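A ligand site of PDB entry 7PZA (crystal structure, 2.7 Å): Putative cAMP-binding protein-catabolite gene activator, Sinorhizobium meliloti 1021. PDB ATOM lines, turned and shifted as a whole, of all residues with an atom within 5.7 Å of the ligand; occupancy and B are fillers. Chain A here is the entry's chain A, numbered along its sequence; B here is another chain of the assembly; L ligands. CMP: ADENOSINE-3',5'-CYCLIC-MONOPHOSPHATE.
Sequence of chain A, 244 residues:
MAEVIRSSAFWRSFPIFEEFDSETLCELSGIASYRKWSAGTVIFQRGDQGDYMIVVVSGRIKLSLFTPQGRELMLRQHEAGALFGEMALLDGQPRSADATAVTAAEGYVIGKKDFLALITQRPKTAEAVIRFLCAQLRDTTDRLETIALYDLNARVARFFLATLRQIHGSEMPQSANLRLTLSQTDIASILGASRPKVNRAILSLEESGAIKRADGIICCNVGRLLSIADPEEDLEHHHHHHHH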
ATOM      1  N   PHE A  44     -28.956  -0.053 -14.229  1.00  0.00           N
ATOM      2  CA  PHE A  44     -28.657  -1.232 -15.035  1.00  0.00           C
ATOM      3  C   PHE A  44     -29.564  -2.389 -14.643  1.00  0.00           C
ATOM      4  O   PHE A  44     -30.269  -2.343 -13.628  1.00  0.00           O
ATOM      5  CB  PHE A  44     -27.170  -1.678 -14.932  1.00  0.00           C
ATOM      6  CG  PHE A  44     -26.625  -1.868 -13.509  1.00  0.00           C
ATOM      7  CD1 PHE A  44     -26.969  -2.981 -12.724  1.00  0.00           C
ATOM      8  CD2 PHE A  44     -25.689  -0.984 -12.987  1.00  0.00           C
ATOM      9  CE1 PHE A  44     -26.443  -3.178 -11.434  1.00  0.00           C
ATOM     10  CE2 PHE A  44     -25.164  -1.184 -11.706  1.00  0.00           C
ATOM     11  CZ  PHE A  44     -25.553  -2.285 -10.937  1.00  0.00           C
ATOM     12  N   GLY A  50     -21.229  -5.289 -16.504  1.00  0.00           N
ATOM     13  CA  GLY A  50     -20.865  -4.258 -15.578  1.00  0.00           C
ATOM     14  C   GLY A  50     -19.382  -3.934 -15.586  1.00  0.00           C
ATOM     15  O   GLY A  50     -18.583  -4.704 -15.010  1.00  0.00           O
ATOM     16  N   LEU A  63     -31.418  -2.063  -5.043  1.00  0.00           N
ATOM     17  CA  LEU A  63     -30.897  -3.268  -5.674  1.00  0.00           C
ATOM     18  C   LEU A  63     -31.846  -4.415  -5.382  1.00  0.00           C
ATOM     19  O   LEU A  63     -32.099  -4.713  -4.210  1.00  0.00           O
ATOM     20  CB  LEU A  63     -29.515  -3.570  -5.135  1.00  0.00           C
ATOM     21  CG  LEU A  63     -28.670  -2.546  -5.836  1.00  0.00           C
ATOM     22  CD1 LEU A  63     -27.887  -1.706  -4.939  1.00  0.00           C
ATOM     23  CD2 LEU A  63     -27.739  -3.388  -6.564  1.00  0.00           C
ATOM     24  N   LEU A  75     -32.900  -6.479  -2.488  1.00  0.00           N
ATOM     25  CA  LEU A  75     -31.639  -6.848  -1.851  1.00  0.00           C
ATOM     26  C   LEU A  75     -31.202  -5.734  -0.911  1.00  0.00           C
ATOM     27  O   LEU A  75     -30.942  -5.995   0.273  1.00  0.00           O
ATOM     28  CB  LEU A  75     -30.552  -7.167  -2.883  1.00  0.00           C
ATOM     29  CG  LEU A  75     -30.516  -8.504  -3.652  1.00  0.00           C
ATOM     30  CD1 LEU A  75     -29.390  -8.542  -4.659  1.00  0.00           C
ATOM     31  CD2 LEU A  75     -30.403  -9.672  -2.647  1.00  0.00           C
ATOM     32  N   ARG A  76     -31.206  -4.482  -1.389  1.00  0.00           N
ATOM     33  CA  ARG A  76     -30.883  -3.362  -0.502  1.00  0.00           C
ATOM     34  C   ARG A  76     -31.546  -2.090  -0.999  1.00  0.00           C
ATOM     35  O   ARG A  76     -31.843  -1.946  -2.183  1.00  0.00           O
ATOM     36  CB  ARG A  76     -29.401  -3.068  -0.469  1.00  0.00           C
ATOM     37  CG  ARG A  76     -28.508  -4.229  -0.317  1.00  0.00           C
ATOM     38  CD  ARG A  76     -28.405  -4.750   1.103  1.00  0.00           C
ATOM     39  NE  ARG A  76     -27.003  -5.011   1.264  1.00  0.00           N
ATOM     40  CZ  ARG A  76     -26.305  -5.089   2.367  1.00  0.00           C
ATOM     41  NH1 ARG A  76     -26.566  -6.026   3.274  1.00  0.00           N
ATOM     42  NH2 ARG A  76     -25.203  -4.322   2.497  1.00  0.00           N
ATOM     43  N   HIS A  78     -30.027   1.570  -0.944  1.00  0.00           N
ATOM     44  CA  HIS A  78     -28.804   2.306  -0.628  1.00  0.00           C
ATOM     45  C   HIS A  78     -29.039   3.800  -0.726  1.00  0.00           C
ATOM     46  O   HIS A  78     -29.711   4.274  -1.654  1.00  0.00           O
ATOM     47  CB  HIS A  78     -27.609   2.009  -1.540  1.00  0.00           C
ATOM     48  CG  HIS A  78     -27.099   0.610  -1.484  1.00  0.00           C
ATOM     49  ND1 HIS A  78     -25.982   0.245  -0.754  1.00  0.00           N
ATOM     50  CD2 HIS A  78     -27.437  -0.473  -2.198  1.00  0.00           C
ATOM     51  CE1 HIS A  78     -25.715  -1.030  -0.961  1.00  0.00           C
ATOM     52  NE2 HIS A  78     -26.578  -1.489  -1.849  1.00  0.00           N
ATOM     53  N   LEU A  83     -22.077   1.683  -1.783  1.00  0.00           N
ATOM     54  CA  LEU A  83     -21.201   1.260  -2.858  1.00  0.00           C
ATOM     55  C   LEU A  83     -21.794   0.020  -3.494  1.00  0.00           C
ATOM     56  O   LEU A  83     -22.108  -0.956  -2.788  1.00  0.00           O
ATOM     57  CB  LEU A  83     -19.815   1.008  -2.292  1.00  0.00           C
ATOM     58  CG  LEU A  83     -18.872   0.668  -3.427  1.00  0.00           C
ATOM     59  CD1 LEU A  83     -17.465   1.266  -3.182  1.00  0.00           C
ATOM     60  CD2 LEU A  83     -18.769  -0.889  -3.623  1.00  0.00           C
ATOM     61  N   PHE A  84     -21.954   0.032  -4.816  1.00  0.00           N
ATOM     62  CA  PHE A  84     -22.657  -1.102  -5.376  1.00  0.00           C
ATOM     63  C   PHE A  84     -22.132  -1.294  -6.820  1.00  0.00           C
ATOM     64  O   PHE A  84     -21.514  -0.403  -7.403  1.00  0.00           O
ATOM     65  CB  PHE A  84     -24.172  -0.869  -5.112  1.00  0.00           C
ATOM     66  CG  PHE A  84     -24.892  -0.038  -6.126  1.00  0.00           C
ATOM     67  CD1 PHE A  84     -24.628  -0.123  -7.484  1.00  0.00           C
ATOM     68  CD2 PHE A  84     -25.676   1.028  -5.686  1.00  0.00           C
ATOM     69  CE1 PHE A  84     -25.288   0.696  -8.411  1.00  0.00           C
ATOM     70  CE2 PHE A  84     -26.322   1.905  -6.634  1.00  0.00           C
ATOM     71  CZ  PHE A  84     -26.107   1.720  -7.995  1.00  0.00           C
ATOM     72  N   GLY A  85     -22.331  -2.467  -7.376  1.00  0.00           N
ATOM     73  CA  GLY A  85     -21.811  -2.721  -8.705  1.00  0.00           C
ATOM     74  C   GLY A  85     -20.369  -3.164  -8.763  1.00  0.00           C
ATOM     75  O   GLY A  85     -19.769  -3.107  -9.829  1.00  0.00           O
ATOM     76  N   GLU A  86     -19.805  -3.621  -7.669  1.00  0.00           N
ATOM     77  CA  GLU A  86     -18.415  -3.988  -7.623  1.00  0.00           C
ATOM     78  C   GLU A  86     -18.176  -5.451  -7.938  1.00  0.00           C
ATOM     79  O   GLU A  86     -17.035  -5.809  -8.194  1.00  0.00           O
ATOM     80  CB  GLU A  86     -17.840  -3.685  -6.236  1.00  0.00           C
ATOM     81  CG  GLU A  86     -18.259  -4.718  -5.215  1.00  0.00           C
ATOM     82  CD  GLU A  86     -19.727  -4.596  -4.843  1.00  0.00           C
ATOM     83  OE1 GLU A  86     -20.384  -3.612  -5.256  1.00  0.00           O
ATOM     84  OE2 GLU A  86     -20.254  -5.517  -4.173  1.00  0.00           O
ATOM     85  N   MET A  87     -19.197  -6.320  -7.895  1.00  0.00           N
ATOM     86  CA  MET A  87     -18.917  -7.740  -8.104  1.00  0.00           C
ATOM     87  C   MET A  87     -18.554  -8.010  -9.555  1.00  0.00           C
ATOM     88  O   MET A  87     -17.527  -8.650  -9.853  1.00  0.00           O
ATOM     89  CB  MET A  87     -20.086  -8.627  -7.706  1.00  0.00           C
ATOM     90  CG  MET A  87     -20.294  -8.767  -6.207  1.00  0.00           C
ATOM     91  SD  MET A  87     -21.937  -9.406  -5.743  1.00  0.00           S
ATOM     92  CE  MET A  87     -21.946 -11.001  -6.564  1.00  0.00           C
ATOM     93  N   ALA A  88     -19.380  -7.530 -10.485  1.00  0.00           N
ATOM     94  CA  ALA A  88     -19.054  -7.710 -11.903  1.00  0.00           C
ATOM     95  C   ALA A  88     -17.796  -6.968 -12.286  1.00  0.00           C
ATOM     96  O   ALA A  88     -17.179  -7.286 -13.318  1.00  0.00           O
ATOM     97  CB  ALA A  88     -20.213  -7.260 -12.766  1.00  0.00           C
ATOM     98  N   LEU A  89     -17.370  -5.984 -11.508  1.00  0.00           N
ATOM     99  CA  LEU A  89     -16.031  -5.440 -11.732  1.00  0.00           C
ATOM    100  C   LEU A  89     -14.959  -6.475 -11.443  1.00  0.00           C
ATOM    101  O   LEU A  89     -14.155  -6.806 -12.318  1.00  0.00           O
ATOM    102  CB  LEU A  89     -15.785  -4.226 -10.857  1.00  0.00           C
ATOM    103  CG  LEU A  89     -15.154  -3.108 -11.639  1.00  0.00           C
ATOM    104  CD1 LEU A  89     -16.120  -2.580 -12.693  1.00  0.00           C
ATOM    105  CD2 LEU A  89     -14.782  -2.066 -10.675  1.00  0.00           C
ATOM    106  N   PRO A  94     -21.571 -11.200 -15.365  1.00  0.00           N
ATOM    107  CA  PRO A  94     -22.546 -10.122 -15.528  1.00  0.00           C
ATOM    108  C   PRO A  94     -23.017  -9.606 -14.171  1.00  0.00           C
ATOM    109  O   PRO A  94     -22.707 -10.196 -13.134  1.00  0.00           O
ATOM    110  CB  PRO A  94     -23.687 -10.784 -16.309  1.00  0.00           C
ATOM    111  CG  PRO A  94     -23.558 -12.205 -16.030  1.00  0.00           C
ATOM    112  CD  PRO A  94     -22.103 -12.472 -15.909  1.00  0.00           C
ATOM    113  N   ARG A  95     -23.758  -8.511 -14.196  1.00  0.00           N
ATOM    114  CA  ARG A  95     -24.408  -7.984 -13.006  1.00  0.00           C
ATOM    115  C   ARG A  95     -25.275  -9.069 -12.367  1.00  0.00           C
ATOM    116  O   ARG A  95     -25.889  -9.896 -13.047  1.00  0.00           O
ATOM    117  CB  ARG A  95     -25.285  -6.798 -13.370  1.00  0.00           C
ATOM    118  CG  ARG A  95     -24.616  -5.685 -14.073  1.00  0.00           C
ATOM    119  CD  ARG A  95     -23.690  -4.972 -13.189  1.00  0.00           C
ATOM    120  NE  ARG A  95     -23.367  -3.638 -13.663  1.00  0.00           N
ATOM    121  CZ  ARG A  95     -22.439  -2.849 -13.142  1.00  0.00           C
ATOM    122  NH1 ARG A  95     -21.670  -3.262 -12.135  1.00  0.00           N
ATOM    123  NH2 ARG A  95     -22.250  -1.638 -13.637  1.00  0.00           N
ATOM    124  N   SER A  96     -25.334  -9.021 -11.061  1.00  0.00           N
ATOM    125  CA  SER A  96     -25.970 -10.024 -10.238  1.00  0.00           C
ATOM    126  C   SER A  96     -27.301  -9.560  -9.656  1.00  0.00           C
ATOM    127  O   SER A  96     -28.057 -10.374  -9.088  1.00  0.00           O
ATOM    128  CB  SER A  96     -24.964 -10.409  -9.171  1.00  0.00           C
ATOM    129  OG  SER A  96     -25.170  -9.555  -8.065  1.00  0.00           O
ATOM    130  N   ALA A  97     -27.633  -8.301  -9.856  1.00  0.00           N
ATOM    131  CA  ALA A  97     -28.917  -7.804  -9.432  1.00  0.00           C
ATOM    132  C   ALA A  97     -29.260  -6.633 -10.316  1.00  0.00           C
ATOM    133  O   ALA A  97     -28.573  -6.320 -11.273  1.00  0.00           O
ATOM    134  CB  ALA A  97     -28.899  -7.411  -7.957  1.00  0.00           C
ATOM    135  N   ASP A  98     -30.326  -5.946  -9.950  1.00  0.00           N
ATOM    136  CA  ASP A  98     -30.942  -4.953 -10.789  1.00  0.00           C
ATOM    137  C   ASP A  98     -30.942  -3.668  -9.959  1.00  0.00           C
ATOM    138  O   ASP A  98     -31.267  -3.703  -8.754  1.00  0.00           O
ATOM    139  CB  ASP A  98     -32.335  -5.478 -11.154  1.00  0.00           C
ATOM    140  CG  ASP A  98     -32.672  -5.311 -12.613  1.00  0.00           C
ATOM    141  OD1 ASP A  98     -32.567  -4.150 -13.076  1.00  0.00           O
ATOM    142  OD2 ASP A  98     -32.974  -6.341 -13.297  1.00  0.00           O
ATOM    143  N   GLN A 136     -20.102  -9.168   3.252  1.00  0.00           N
ATOM    144  CA  GLN A 136     -21.323  -9.427   2.485  1.00  0.00           C
ATOM    145  C   GLN A 136     -21.767 -10.878   2.614  1.00  0.00           C
ATOM    146  O   GLN A 136     -22.916 -11.174   2.992  1.00  0.00           O
ATOM    147  CB  GLN A 136     -21.133  -9.079   1.024  1.00  0.00           C
ATOM    148  CG  GLN A 136     -20.751  -7.646   0.699  1.00  0.00           C
ATOM    149  CD  GLN A 136     -21.767  -6.630   1.148  1.00  0.00           C
ATOM    150  OE1 GLN A 136     -22.516  -6.844   2.068  1.00  0.00           O
ATOM    151  NE2 GLN A 136     -21.885  -5.558   0.396  1.00  0.00           N
ATOM    152  N   THR A 140     -25.273 -12.145   3.904  1.00  0.00           N
ATOM    153  CA  THR A 140     -26.240 -12.797   3.031  1.00  0.00           C
ATOM    154  C   THR A 140     -26.607 -14.166   3.578  1.00  0.00           C
ATOM    155  O   THR A 140     -27.798 -14.507   3.659  1.00  0.00           O
ATOM    156  CB  THR A 140     -25.701 -12.853   1.619  1.00  0.00           C
ATOM    157  OG1 THR A 140     -25.066 -11.611   1.352  1.00  0.00           O
ATOM    158  CG2 THR A 140     -26.871 -12.957   0.678  1.00  0.00           C
ATOM    159  N   ARG A 143     -29.151 -13.660   6.290  1.00  0.00           N
ATOM    160  CA  ARG A 143     -30.433 -13.499   5.623  1.00  0.00           C
ATOM    161  C   ARG A 143     -31.026 -14.840   5.262  1.00  0.00           C
ATOM    162  O   ARG A 143     -32.212 -15.100   5.519  1.00  0.00           O
ATOM    163  CB  ARG A 143     -30.246 -12.624   4.410  1.00  0.00           C
ATOM    164  CG  ARG A 143     -31.479 -12.255   3.618  1.00  0.00           C
ATOM    165  CD  ARG A 143     -31.654 -10.795   3.751  1.00  0.00           C
ATOM    166  NE  ARG A 143     -31.019 -10.144   2.640  1.00  0.00           N
ATOM    167  CZ  ARG A 143     -31.503  -9.199   1.884  1.00  0.00           C
ATOM    168  NH1 ARG A 143     -32.819  -9.090   1.675  1.00  0.00           N
ATOM    169  NH2 ARG A 143     -30.666  -8.372   1.264  1.00  0.00           N
ATOM    170  N   LEU B 137     -20.510 -15.429  -2.947  1.00  0.00           N
ATOM    171  CA  LEU B 137     -21.580 -14.460  -2.802  1.00  0.00           C
ATOM    172  C   LEU B 137     -22.683 -14.709  -3.831  1.00  0.00           C
ATOM    173  O   LEU B 137     -23.851 -14.793  -3.470  1.00  0.00           O
ATOM    174  CB  LEU B 137     -20.986 -13.052  -2.908  1.00  0.00           C
ATOM    175  CG  LEU B 137     -21.845 -11.986  -2.293  1.00  0.00           C
ATOM    176  CD1 LEU B 137     -22.294 -12.466  -0.963  1.00  0.00           C
ATOM    177  CD2 LEU B 137     -21.021 -10.783  -2.161  1.00  0.00           C
ATOM    178  N   ARG B 138     -22.289 -14.974  -5.088  1.00  0.00           N
ATOM    179  CA  ARG B 138     -23.290 -15.277  -6.121  1.00  0.00           C
ATOM    180  C   ARG B 138     -24.059 -16.525  -5.762  1.00  0.00           C
ATOM    181  O   ARG B 138     -25.289 -16.490  -5.625  1.00  0.00           O
ATOM    182  CB  ARG B 138     -22.601 -15.469  -7.471  1.00  0.00           C
ATOM    183  CG  ARG B 138     -22.071 -14.195  -8.034  1.00  0.00           C
ATOM    184  CD  ARG B 138     -21.250 -14.370  -9.288  1.00  0.00           C
ATOM    185  NE  ARG B 138     -20.556 -13.141  -9.616  1.00  0.00           N
ATOM    186  CZ  ARG B 138     -21.150 -12.142 -10.259  1.00  0.00           C
ATOM    187  NH1 ARG B 138     -22.383 -12.268 -10.733  1.00  0.00           N
ATOM    188  NH2 ARG B 138     -20.493 -10.999 -10.436  1.00  0.00           N
ATOM    189  N   THR B 141     -26.465 -15.771  -2.950  1.00  0.00           N
ATOM    190  CA  THR B 141     -27.634 -15.003  -3.342  1.00  0.00           C
ATOM    191  C   THR B 141     -28.523 -15.815  -4.257  1.00  0.00           C
ATOM    192  O   THR B 141     -29.745 -15.677  -4.164  1.00  0.00           O
ATOM    193  CB  THR B 141     -27.256 -13.661  -3.989  1.00  0.00           C
ATOM    194  OG1 THR B 141     -26.083 -13.824  -4.788  1.00  0.00           O
ATOM    195  CG2 THR B 141     -26.802 -12.766  -2.945  1.00  0.00           C
HETATM  196  P   CMP L   1     -23.067  -6.215  -9.332  1.00  0.00           P
HETATM  197  O1P CMP L   1     -22.140  -5.620 -10.327  1.00  0.00           O
HETATM  198  O2P CMP L   1     -23.303  -7.702  -9.287  1.00  0.00           O
HETATM  199  O5' CMP L   1     -24.541  -5.715  -9.656  1.00  0.00           O
HETATM  200  C5' CMP L   1     -25.580  -5.860  -8.697  1.00  0.00           C
HETATM  201  C4' CMP L   1     -25.069  -5.378  -7.393  1.00  0.00           C
HETATM  202  O4' CMP L   1     -25.943  -5.681  -6.304  1.00  0.00           O
HETATM  203  C3' CMP L   1     -23.789  -6.040  -6.991  1.00  0.00           C
HETATM  204  O3' CMP L   1     -22.744  -5.646  -7.845  1.00  0.00           O
HETATM  205  C2' CMP L   1     -23.692  -5.676  -5.535  1.00  0.00           C
HETATM  206  O2' CMP L   1     -23.240  -4.336  -5.357  1.00  0.00           O
HETATM  207  C1' CMP L   1     -25.176  -5.784  -5.123  1.00  0.00           C
HETATM  208  N9  CMP L   1     -25.444  -7.090  -4.531  1.00  0.00           N
HETATM  209  C8  CMP L   1     -25.437  -8.289  -5.132  1.00  0.00           C
HETATM  210  N7  CMP L   1     -25.659  -9.278  -4.239  1.00  0.00           N
HETATM  211  C5  CMP L   1     -25.817  -8.683  -3.033  1.00  0.00           C
HETATM  212  C6  CMP L   1     -26.069  -9.074  -1.632  1.00  0.00           C
HETATM  213  N6  CMP L   1     -26.224 -10.352  -1.273  1.00  0.00           N
HETATM  214  N1  CMP L   1     -26.126  -8.134  -0.677  1.00  0.00           N
HETATM  215  C2  CMP L   1     -25.968  -6.837  -0.968  1.00  0.00           C
HETATM  216  N3  CMP L   1     -25.733  -6.381  -2.205  1.00  0.00           N
HETATM  217  C4  CMP L   1     -25.657  -7.240  -3.251  1.00  0.00           C
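An oxygen (O2') of the ligand is in hydrogen-bond range of the backbone NH (N) of Gly 85, at 2.9 Å.
The backbone NH of Ser 96 is in hydrogen-bond range of an oxygen (O2P) of the ligand (3.0 Å).
O2P of the ligand is in hydrogen-bond range of OG of Ser 96, at 2.9 Å.
The side-chain carboxylate of Glu 86 is in hydrogen-bond range of an oxygen (O2') of the ligand, at 2.9 Å.
The guanidinium group of Arg 95 is in salt-bridge range of an oxygen (O1P) of the ligand (3.0 Å).
N6 of the ligand lies within hydrogen-bond range of OG1 of Thr 140 (3.1 Å).
N of Ala 88 is in hydrogen-bond range of O1P of the ligand (3.4 Å).
Phe 44 touches the ligand.
Leu 63 touches the ligand (CD2 to O4', 2.9 Å).
Leu 75 touches the ligand (CD1 to N7, 3.8 Å).
NE of Arg 76 touches C2 of the ligand, at 3.1 Å.
Phe 84 touches the ligand.
Met 87 touches the ligand.
Ala 97 touches the ligand (N to C5', 3.4 Å).
Thr 141 of chain B touches the ligand.
Hydrophobic or aromatic side chains that line the ligand: Phe 44, Leu 63, Leu 75, Phe 84, Met 87, Ala 88 and Ala 97.
Within 4 Å of the ligand: Phe 44, Leu 63, Leu 75, Arg 76, Phe 84, Gly 85, Glu 86, Met 87, Ala 88, Arg 95, Ser 96, Ala 97, Thr 140 and Thr 141 of chain B.
The guanidinium group (NH1) of Arg 95 lies within hydrogen-bond range of the backbone carbonyl oxygen (O) of Gly 85.
O of Arg 76 sits at hydrogen-bond distance from N of Leu 63 (2.9 Å).
The backbone NH of Leu 75 sits at hydrogen-bond distance from the backbone carbonyl oxygen of Leu 63 (2.6 Å).
OG1 of Thr 141 of chain B sits at hydrogen-bond distance from O of Leu 137 of chain B (2.8 Å).
The side-chain hydroxyl of Thr 141 of chain B lies within hydrogen-bond range of the backbone carbonyl oxygen of Arg 138 of chain B (2.9 Å).
OG1 of Thr 140 sits at hydrogen-bond distance from O of Gln 136 (2.7 Å).
The guanidinium group (NH2) of Arg 143 sits at hydrogen-bond distance from the backbone carbonyl oxygen (O) of Leu 75 (2.6 Å).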
